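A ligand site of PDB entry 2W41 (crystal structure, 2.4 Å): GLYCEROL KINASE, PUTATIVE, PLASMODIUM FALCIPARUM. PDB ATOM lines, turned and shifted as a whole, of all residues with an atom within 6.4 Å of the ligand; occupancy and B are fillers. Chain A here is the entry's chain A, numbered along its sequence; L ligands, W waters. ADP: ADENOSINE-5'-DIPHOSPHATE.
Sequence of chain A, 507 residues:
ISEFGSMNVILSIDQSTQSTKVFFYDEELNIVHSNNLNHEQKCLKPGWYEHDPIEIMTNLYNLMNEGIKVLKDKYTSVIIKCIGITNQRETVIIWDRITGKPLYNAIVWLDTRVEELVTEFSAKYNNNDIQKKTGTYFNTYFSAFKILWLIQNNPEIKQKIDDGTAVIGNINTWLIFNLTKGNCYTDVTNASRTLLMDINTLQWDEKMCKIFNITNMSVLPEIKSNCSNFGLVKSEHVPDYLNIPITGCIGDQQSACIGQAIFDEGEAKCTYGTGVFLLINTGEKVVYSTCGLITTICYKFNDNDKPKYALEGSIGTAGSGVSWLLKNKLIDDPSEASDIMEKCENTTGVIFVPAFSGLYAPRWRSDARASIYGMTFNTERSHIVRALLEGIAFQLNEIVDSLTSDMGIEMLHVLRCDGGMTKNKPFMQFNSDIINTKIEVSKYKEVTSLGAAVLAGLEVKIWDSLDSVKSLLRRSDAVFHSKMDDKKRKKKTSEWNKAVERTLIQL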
ATOM      1  N   THR A 271      19.979  -3.280  -9.271  1.00  0.00           N
ATOM      2  CA  THR A 271      21.144  -2.617  -9.868  1.00  0.00           C
ATOM      3  C   THR A 271      21.792  -3.514 -10.945  1.00  0.00           C
ATOM      4  O   THR A 271      22.121  -4.683 -10.665  1.00  0.00           O
ATOM      5  CB  THR A 271      22.168  -2.205  -8.759  1.00  0.00           C
ATOM      6  OG1 THR A 271      21.567  -1.243  -7.865  1.00  0.00           O
ATOM      7  CG2 THR A 271      23.476  -1.635  -9.340  1.00  0.00           C
ATOM      8  N   TYR A 272      21.984  -3.011 -12.165  1.00  0.00           N
ATOM      9  CA  TYR A 272      22.764  -3.776 -13.160  1.00  0.00           C
ATOM     10  C   TYR A 272      24.115  -3.151 -13.478  1.00  0.00           C
ATOM     11  O   TYR A 272      24.284  -2.538 -14.528  1.00  0.00           O
ATOM     12  CB  TYR A 272      22.034  -3.917 -14.484  1.00  0.00           C
ATOM     13  CG  TYR A 272      20.728  -4.654 -14.505  1.00  0.00           C
ATOM     14  CD1 TYR A 272      20.637  -5.932 -14.797  1.00  0.00           C
ATOM     15  CD2 TYR A 272      19.585  -4.049 -14.318  1.00  0.00           C
ATOM     16  CE1 TYR A 272      19.420  -6.593 -14.840  1.00  0.00           C
ATOM     17  CE2 TYR A 272      18.371  -4.731 -14.373  1.00  0.00           C
ATOM     18  CZ  TYR A 272      18.299  -5.989 -14.653  1.00  0.00           C
ATOM     19  OH  TYR A 272      17.095  -6.647 -14.699  1.00  0.00           O
ATOM     20  N   GLY A 273      25.068  -3.317 -12.573  1.00  0.00           N
ATOM     21  CA  GLY A 273      26.445  -2.863 -12.771  1.00  0.00           C
ATOM     22  C   GLY A 273      27.389  -4.055 -12.947  1.00  0.00           C
ATOM     23  O   GLY A 273      26.977  -5.106 -13.448  1.00  0.00           O
ATOM     24  N   THR A 274      28.645  -3.874 -12.555  1.00  0.00           N
ATOM     25  CA  THR A 274      29.548  -4.986 -12.376  1.00  0.00           C
ATOM     26  C   THR A 274      28.864  -6.091 -11.546  1.00  0.00           C
ATOM     27  O   THR A 274      28.883  -7.263 -11.944  1.00  0.00           O
ATOM     28  CB  THR A 274      30.864  -4.509 -11.758  1.00  0.00           C
ATOM     29  OG1 THR A 274      31.453  -3.599 -12.672  1.00  0.00           O
ATOM     30  CG2 THR A 274      31.874  -5.645 -11.550  1.00  0.00           C
ATOM     31  N   GLY A 275      28.237  -5.721 -10.435  1.00  0.00           N
ATOM     32  CA  GLY A 275      27.400  -6.628  -9.698  1.00  0.00           C
ATOM     33  C   GLY A 275      25.961  -6.444 -10.131  1.00  0.00           C
ATOM     34  O   GLY A 275      25.570  -5.353 -10.525  1.00  0.00           O
ATOM     35  N   ALA A 318      27.924 -10.525 -12.372  1.00  0.00           N
ATOM     36  CA  ALA A 318      27.321 -10.785 -13.722  1.00  0.00           C
ATOM     37  C   ALA A 318      27.658  -9.775 -14.830  1.00  0.00           C
ATOM     38  O   ALA A 318      27.893 -10.182 -15.953  1.00  0.00           O
ATOM     39  CB  ALA A 318      25.857 -10.978 -13.620  1.00  0.00           C
ATOM     40  N   GLY A 319      27.706  -8.481 -14.510  1.00  0.00           N
ATOM     41  CA  GLY A 319      28.093  -7.454 -15.483  1.00  0.00           C
ATOM     42  C   GLY A 319      29.524  -7.614 -15.976  1.00  0.00           C
ATOM     43  O   GLY A 319      29.891  -7.136 -17.047  1.00  0.00           O
ATOM     44  N   SER A 320      30.355  -8.292 -15.192  1.00  0.00           N
ATOM     45  CA  SER A 320      31.695  -8.632 -15.688  1.00  0.00           C
ATOM     46  C   SER A 320      31.761  -9.629 -16.845  1.00  0.00           C
ATOM     47  O   SER A 320      32.825  -9.803 -17.420  1.00  0.00           O
ATOM     48  CB  SER A 320      32.604  -9.094 -14.570  1.00  0.00           C
ATOM     49  OG  SER A 320      32.914  -7.970 -13.772  1.00  0.00           O
ATOM     50  N   GLY A 321      30.655 -10.308 -17.145  1.00  0.00           N
ATOM     51  CA  GLY A 321      30.568 -11.158 -18.301  1.00  0.00           C
ATOM     52  C   GLY A 321      30.633 -10.349 -19.581  1.00  0.00           C
ATOM     53  O   GLY A 321      31.079 -10.869 -20.626  1.00  0.00           O
ATOM     54  N   VAL A 322      30.153  -9.099 -19.532  1.00  0.00           N
ATOM     55  CA  VAL A 322      30.416  -8.142 -20.631  1.00  0.00           C
ATOM     56  C   VAL A 322      31.904  -7.799 -20.812  1.00  0.00           C
ATOM     57  O   VAL A 322      32.390  -7.797 -21.926  1.00  0.00           O
ATOM     58  CB  VAL A 322      29.580  -6.868 -20.561  1.00  0.00           C
ATOM     59  CG1 VAL A 322      29.966  -5.948 -21.682  1.00  0.00           C
ATOM     60  CG2 VAL A 322      28.093  -7.207 -20.653  1.00  0.00           C
ATOM     61  N   SER A 323      32.640  -7.558 -19.720  1.00  0.00           N
ATOM     62  CA  SER A 323      34.104  -7.476 -19.765  1.00  0.00           C
ATOM     63  C   SER A 323      34.818  -8.730 -20.311  1.00  0.00           C
ATOM     64  O   SER A 323      35.865  -8.609 -20.959  1.00  0.00           O
ATOM     65  CB  SER A 323      34.686  -7.131 -18.379  1.00  0.00           C
ATOM     66  OG  SER A 323      33.785  -6.310 -17.653  1.00  0.00           O
ATOM     67  N   LEU A 326      34.664  -8.830 -24.005  1.00  0.00           N
ATOM     68  CA  LEU A 326      35.680  -7.859 -24.448  1.00  0.00           C
ATOM     69  C   LEU A 326      37.107  -8.432 -24.377  1.00  0.00           C
ATOM     70  O   LEU A 326      37.891  -8.272 -25.321  1.00  0.00           O
ATOM     71  CB  LEU A 326      35.602  -6.579 -23.594  1.00  0.00           C
ATOM     72  CG  LEU A 326      34.620  -5.436 -23.921  1.00  0.00           C
ATOM     73  CD1 LEU A 326      34.672  -4.467 -22.802  1.00  0.00           C
ATOM     74  CD2 LEU A 326      34.964  -4.697 -25.182  1.00  0.00           C
ATOM     75  N   PRO A 334      31.483  -2.048 -24.913  1.00  0.00           N
ATOM     76  CA  PRO A 334      30.206  -2.334 -24.278  1.00  0.00           C
ATOM     77  C   PRO A 334      28.987  -1.805 -25.039  1.00  0.00           C
ATOM     78  O   PRO A 334      27.901  -2.370 -24.926  1.00  0.00           O
ATOM     79  CB  PRO A 334      30.329  -1.606 -22.926  1.00  0.00           C
ATOM     80  CG  PRO A 334      31.755  -1.620 -22.625  1.00  0.00           C
ATOM     81  CD  PRO A 334      32.457  -1.483 -23.958  1.00  0.00           C
ATOM     82  N   SER A 335      29.161  -0.728 -25.787  1.00  0.00           N
ATOM     83  CA  SER A 335      28.039  -0.095 -26.485  1.00  0.00           C
ATOM     84  C   SER A 335      27.547  -0.986 -27.605  1.00  0.00           C
ATOM     85  O   SER A 335      26.347  -1.021 -27.906  1.00  0.00           O
ATOM     86  CB  SER A 335      28.376   1.341 -26.967  1.00  0.00           C
ATOM     87  OG  SER A 335      28.980   1.372 -28.250  1.00  0.00           O
ATOM     88  N   GLU A 336      28.485  -1.742 -28.175  1.00  0.00           N
ATOM     89  CA  GLU A 336      28.209  -2.765 -29.173  1.00  0.00           C
ATOM     90  C   GLU A 336      27.233  -3.858 -28.670  1.00  0.00           C
ATOM     91  O   GLU A 336      26.671  -4.588 -29.486  1.00  0.00           O
ATOM     92  CB  GLU A 336      29.518  -3.396 -29.572  1.00  0.00           C
ATOM     93  CG  GLU A 336      29.581  -4.078 -30.937  1.00  0.00           C
ATOM     94  CD  GLU A 336      30.938  -4.771 -31.160  1.00  0.00           C
ATOM     95  OE1 GLU A 336      32.003  -4.177 -30.870  1.00  0.00           O
ATOM     96  OE2 GLU A 336      30.947  -5.937 -31.606  1.00  0.00           O
ATOM     97  N   ALA A 337      27.042  -3.983 -27.353  1.00  0.00           N
ATOM     98  CA  ALA A 337      26.124  -4.956 -26.780  1.00  0.00           C
ATOM     99  C   ALA A 337      24.648  -4.532 -26.985  1.00  0.00           C
ATOM    100  O   ALA A 337      23.763  -5.368 -27.252  1.00  0.00           O
ATOM    101  CB  ALA A 337      26.438  -5.138 -25.284  1.00  0.00           C
ATOM    102  N   SER A 338      24.399  -3.224 -26.857  1.00  0.00           N
ATOM    103  CA  SER A 338      23.103  -2.638 -27.202  1.00  0.00           C
ATOM    104  C   SER A 338      22.727  -2.856 -28.667  1.00  0.00           C
ATOM    105  O   SER A 338      21.604  -3.260 -28.985  1.00  0.00           O
ATOM    106  CB  SER A 338      23.107  -1.146 -26.903  1.00  0.00           C
ATOM    107  OG  SER A 338      23.521  -0.885 -25.576  1.00  0.00           O
ATOM    108  N   LEU A 389      23.928 -12.276 -22.311  1.00  0.00           N
ATOM    109  CA  LEU A 389      23.018 -11.273 -21.758  1.00  0.00           C
ATOM    110  C   LEU A 389      21.682 -11.851 -21.340  1.00  0.00           C
ATOM    111  O   LEU A 389      21.165 -11.571 -20.268  1.00  0.00           O
ATOM    112  CB  LEU A 389      22.818 -10.143 -22.781  1.00  0.00           C
ATOM    113  CG  LEU A 389      24.048  -9.234 -22.912  1.00  0.00           C
ATOM    114  CD1 LEU A 389      23.888  -8.287 -24.147  1.00  0.00           C
ATOM    115  CD2 LEU A 389      24.305  -8.478 -21.594  1.00  0.00           C
ATOM    116  N   ASP A 418      18.773   0.548 -12.067  1.00  0.00           N
ATOM    117  CA  ASP A 418      19.851   1.454 -12.300  1.00  0.00           C
ATOM    118  C   ASP A 418      21.115   0.655 -12.676  1.00  0.00           C
ATOM    119  O   ASP A 418      21.054  -0.580 -12.834  1.00  0.00           O
ATOM    120  CB  ASP A 418      20.017   2.420 -11.130  1.00  0.00           C
ATOM    121  CG  ASP A 418      20.119   1.725  -9.762  1.00  0.00           C
ATOM    122  OD1 ASP A 418      19.049   1.429  -9.101  1.00  0.00           O
ATOM    123  OD2 ASP A 418      21.265   1.529  -9.326  1.00  0.00           O
ATOM    124  N   GLY A 419      22.220   1.388 -12.911  1.00  0.00           N
ATOM    125  CA  GLY A 419      23.473   0.831 -13.356  1.00  0.00           C
ATOM    126  C   GLY A 419      23.600   0.886 -14.870  1.00  0.00           C
ATOM    127  O   GLY A 419      22.618   1.089 -15.601  1.00  0.00           O
ATOM    128  N   GLY A 420      24.817   0.654 -15.334  1.00  0.00           N
ATOM    129  CA  GLY A 420      25.203   0.871 -16.711  1.00  0.00           C
ATOM    130  C   GLY A 420      24.602  -0.042 -17.735  1.00  0.00           C
ATOM    131  O   GLY A 420      24.473   0.352 -18.878  1.00  0.00           O
ATOM    132  N   MET A 421      24.247  -1.252 -17.334  1.00  0.00           N
ATOM    133  CA  MET A 421      23.554  -2.190 -18.248  1.00  0.00           C
ATOM    134  C   MET A 421      22.144  -1.671 -18.654  1.00  0.00           C
ATOM    135  O   MET A 421      21.573  -2.133 -19.653  1.00  0.00           O
ATOM    136  CB  MET A 421      23.464  -3.599 -17.627  1.00  0.00           C
ATOM    137  CG  MET A 421      24.792  -4.290 -17.364  1.00  0.00           C
ATOM    138  SD  MET A 421      24.646  -6.071 -17.008  1.00  0.00           S
ATOM    139  CE  MET A 421      24.492  -6.694 -18.672  1.00  0.00           C
ATOM    140  N   THR A 422      21.601  -0.727 -17.868  1.00  0.00           N
ATOM    141  CA  THR A 422      20.281  -0.130 -18.127  1.00  0.00           C
ATOM    142  C   THR A 422      20.223   0.851 -19.330  1.00  0.00           C
ATOM    143  O   THR A 422      19.146   1.292 -19.716  1.00  0.00           O
ATOM    144  CB  THR A 422      19.650   0.576 -16.885  1.00  0.00           C
ATOM    145  OG1 THR A 422      20.483   1.672 -16.490  1.00  0.00           O
ATOM    146  CG2 THR A 422      19.420  -0.388 -15.740  1.00  0.00           C
ATOM    147  N   LYS A 423      21.394   1.194 -19.864  1.00  0.00           N
ATOM    148  CA  LYS A 423      21.532   1.931 -21.122  1.00  0.00           C
ATOM    149  C   LYS A 423      21.221   1.045 -22.336  1.00  0.00           C
ATOM    150  O   LYS A 423      20.895   1.552 -23.401  1.00  0.00           O
ATOM    151  CB  LYS A 423      22.953   2.502 -21.248  1.00  0.00           C
ATOM    152  CG  LYS A 423      23.098   3.913 -20.657  1.00  0.00           C
ATOM    153  CD  LYS A 423      22.149   4.956 -21.408  1.00  0.00           C
ATOM    154  CE  LYS A 423      21.637   6.139 -20.510  1.00  0.00           C
ATOM    155  NZ  LYS A 423      20.523   6.909 -21.188  1.00  0.00           N
ATOM    156  N   ASN A 424      21.320  -0.256 -22.153  1.00  0.00           N
ATOM    157  CA  ASN A 424      20.928  -1.215 -23.144  1.00  0.00           C
ATOM    158  C   ASN A 424      19.411  -1.441 -23.089  1.00  0.00           C
ATOM    159  O   ASN A 424      18.920  -2.169 -22.207  1.00  0.00           O
ATOM    160  CB  ASN A 424      21.688  -2.522 -22.865  1.00  0.00           C
ATOM    161  CG  ASN A 424      21.676  -3.459 -24.048  1.00  0.00           C
ATOM    162  OD1 ASN A 424      22.674  -4.085 -24.362  1.00  0.00           O
ATOM    163  ND2 ASN A 424      20.532  -3.567 -24.698  1.00  0.00           N
ATOM    164  N   PHE A 427      18.095  -5.097 -23.989  1.00  0.00           N
ATOM    165  CA  PHE A 427      18.344  -5.924 -22.788  1.00  0.00           C
ATOM    166  C   PHE A 427      17.354  -5.682 -21.610  1.00  0.00           C
ATOM    167  O   PHE A 427      16.899  -6.644 -20.993  1.00  0.00           O
ATOM    168  CB  PHE A 427      19.822  -5.811 -22.364  1.00  0.00           C
ATOM    169  CG  PHE A 427      20.144  -6.466 -21.030  1.00  0.00           C
ATOM    170  CD1 PHE A 427      20.257  -7.874 -20.906  1.00  0.00           C
ATOM    171  CD2 PHE A 427      20.354  -5.668 -19.878  1.00  0.00           C
ATOM    172  CE1 PHE A 427      20.557  -8.461 -19.685  1.00  0.00           C
ATOM    173  CE2 PHE A 427      20.654  -6.251 -18.648  1.00  0.00           C
ATOM    174  CZ  PHE A 427      20.767  -7.648 -18.552  1.00  0.00           C
HETATM  175  PB  ADP L   1      29.739  -0.532 -11.343  1.00  0.00           P
HETATM  176  O1B ADP L   1      31.057  -1.280 -11.287  1.00  0.00           O
HETATM  177  O2B ADP L   1      29.928   0.925 -10.971  1.00  0.00           O
HETATM  178  O3B ADP L   1      28.582  -1.226 -10.629  1.00  0.00           O
HETATM  179  PA  ADP L   1      28.279   0.505 -13.705  1.00  0.00           P
HETATM  180  O1A ADP L   1      29.053   1.787 -14.023  1.00  0.00           O
HETATM  181  O2A ADP L   1      26.930   0.585 -13.030  1.00  0.00           O
HETATM  182  O3A ADP L   1      29.320  -0.501 -12.923  1.00  0.00           O
HETATM  183  O5' ADP L   1      28.101  -0.305 -15.102  1.00  0.00           O
HETATM  184  C5' ADP L   1      29.233  -0.930 -15.684  1.00  0.00           C
HETATM  185  C4' ADP L   1      28.828  -2.353 -16.027  1.00  0.00           C
HETATM  186  O4' ADP L   1      27.856  -2.276 -17.066  1.00  0.00           O
HETATM  187  C3' ADP L   1      29.931  -3.177 -16.629  1.00  0.00           C
HETATM  188  O3' ADP L   1      29.584  -4.516 -16.309  1.00  0.00           O
HETATM  189  C2' ADP L   1      29.734  -2.989 -18.124  1.00  0.00           C
HETATM  190  O2' ADP L   1      30.345  -4.002 -18.912  1.00  0.00           O
HETATM  191  C1' ADP L   1      28.237  -2.997 -18.240  1.00  0.00           C
HETATM  192  N9  ADP L   1      27.701  -2.306 -19.443  1.00  0.00           N
HETATM  193  C8  ADP L   1      28.004  -1.035 -19.770  1.00  0.00           C
HETATM  194  N7  ADP L   1      27.393  -0.673 -20.923  1.00  0.00           N
HETATM  195  C5  ADP L   1      26.666  -1.711 -21.354  1.00  0.00           C
HETATM  196  C6  ADP L   1      25.788  -1.946 -22.520  1.00  0.00           C
HETATM  197  N6  ADP L   1      25.614  -0.931 -23.395  1.00  0.00           N
HETATM  198  N1  ADP L   1      25.200  -3.170 -22.638  1.00  0.00           N
HETATM  199  C2  ADP L   1      25.417  -4.156 -21.736  1.00  0.00           C
HETATM  200  N3  ADP L   1      26.233  -4.010 -20.656  1.00  0.00           N
HETATM  201  C4  ADP L   1      26.861  -2.808 -20.393  1.00  0.00           C
HETATM  202  O   HOH W   1      25.618   1.952 -24.222  1.00  0.00           O
HETATM  203  O   HOH W   2      29.771   3.668 -11.692  1.00  0.00           O
HETATM  204  O   HOH W   3      32.653  -4.657 -14.918  1.00  0.00           O
HETATM  205  O   HOH W   4      27.884  -3.163  -8.432  1.00  0.00           O
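O of Pro 334 is in hydrogen-bond range of N6 of the ligand (3.1 Å). N of Gly 420 is in hydrogen-bond range of O2A of the ligand (3.1 Å). An oxygen (O3') of the ligand sits at hydrogen-bond distance from the backbone carbonyl oxygen (O) of Gly 319. N6 of the ligand is in hydrogen-bond range of OG of Ser 338 (3.0 Å). A nitrogen (N1) of the ligand lies close to the side-chain amide oxygen of Asn 424, at 3.2 Å. O3B of the ligand is in hydrogen-bond range of N of Thr 274 (3.3 Å). The side-chain hydroxyl (OG1) of Thr 274 is in hydrogen-bond range of an oxygen (O1B) of the ligand, at 2.7 Å.
N of Ser 338 is in hydrogen-bond range of OD1 of Asn 424. N of Gly 420 sits at hydrogen-bond distance from O of Tyr 272, at 3.3 Å. The side-chain amide nitrogen (ND2) of Asn 424 lies close to the backbone NH (N) of Phe 427, at 3.0 Å. O of Thr 274 sits at hydrogen-bond distance from N of Gly 319, 3.1 Å away. O of Tyr 272 sits at hydrogen-bond distance from N of Met 421. OD1 of Asn 424 sits close to O of Ala 337. O of Thr 274 sits at hydrogen-bond distance from N of Ala 318, at 3.4 Å.
Gly 273 touches the ligand. CB of Val 322 touches O2' of the ligand (3.4 Å). Ala 337 touches the ligand (CB to N1, 3.5 Å). CA of Gly 419 touches O2A of the ligand, at 3.5 Å. Met 421 touches the ligand. Hydrophobic or aromatic side chains that line the ligand: Val 322, Pro 334, Ala 337 and Met 421. The nearest printed residue that does not touch the ligand is Ser 320 (4.01 Å).
Water W4 bridges an oxygen (O3B) of the ligand (3.0 Å) and the backbone NH of Gly 275 (3.3 Å). Water W3 lies within hydrogen-bond range of the side-chain hydroxyl of Thr 274 (2.8 Å), an oxygen (O3') of the ligand (3.4 Å) and the side-chain hydroxyl of Ser 323 (3.4 Å).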
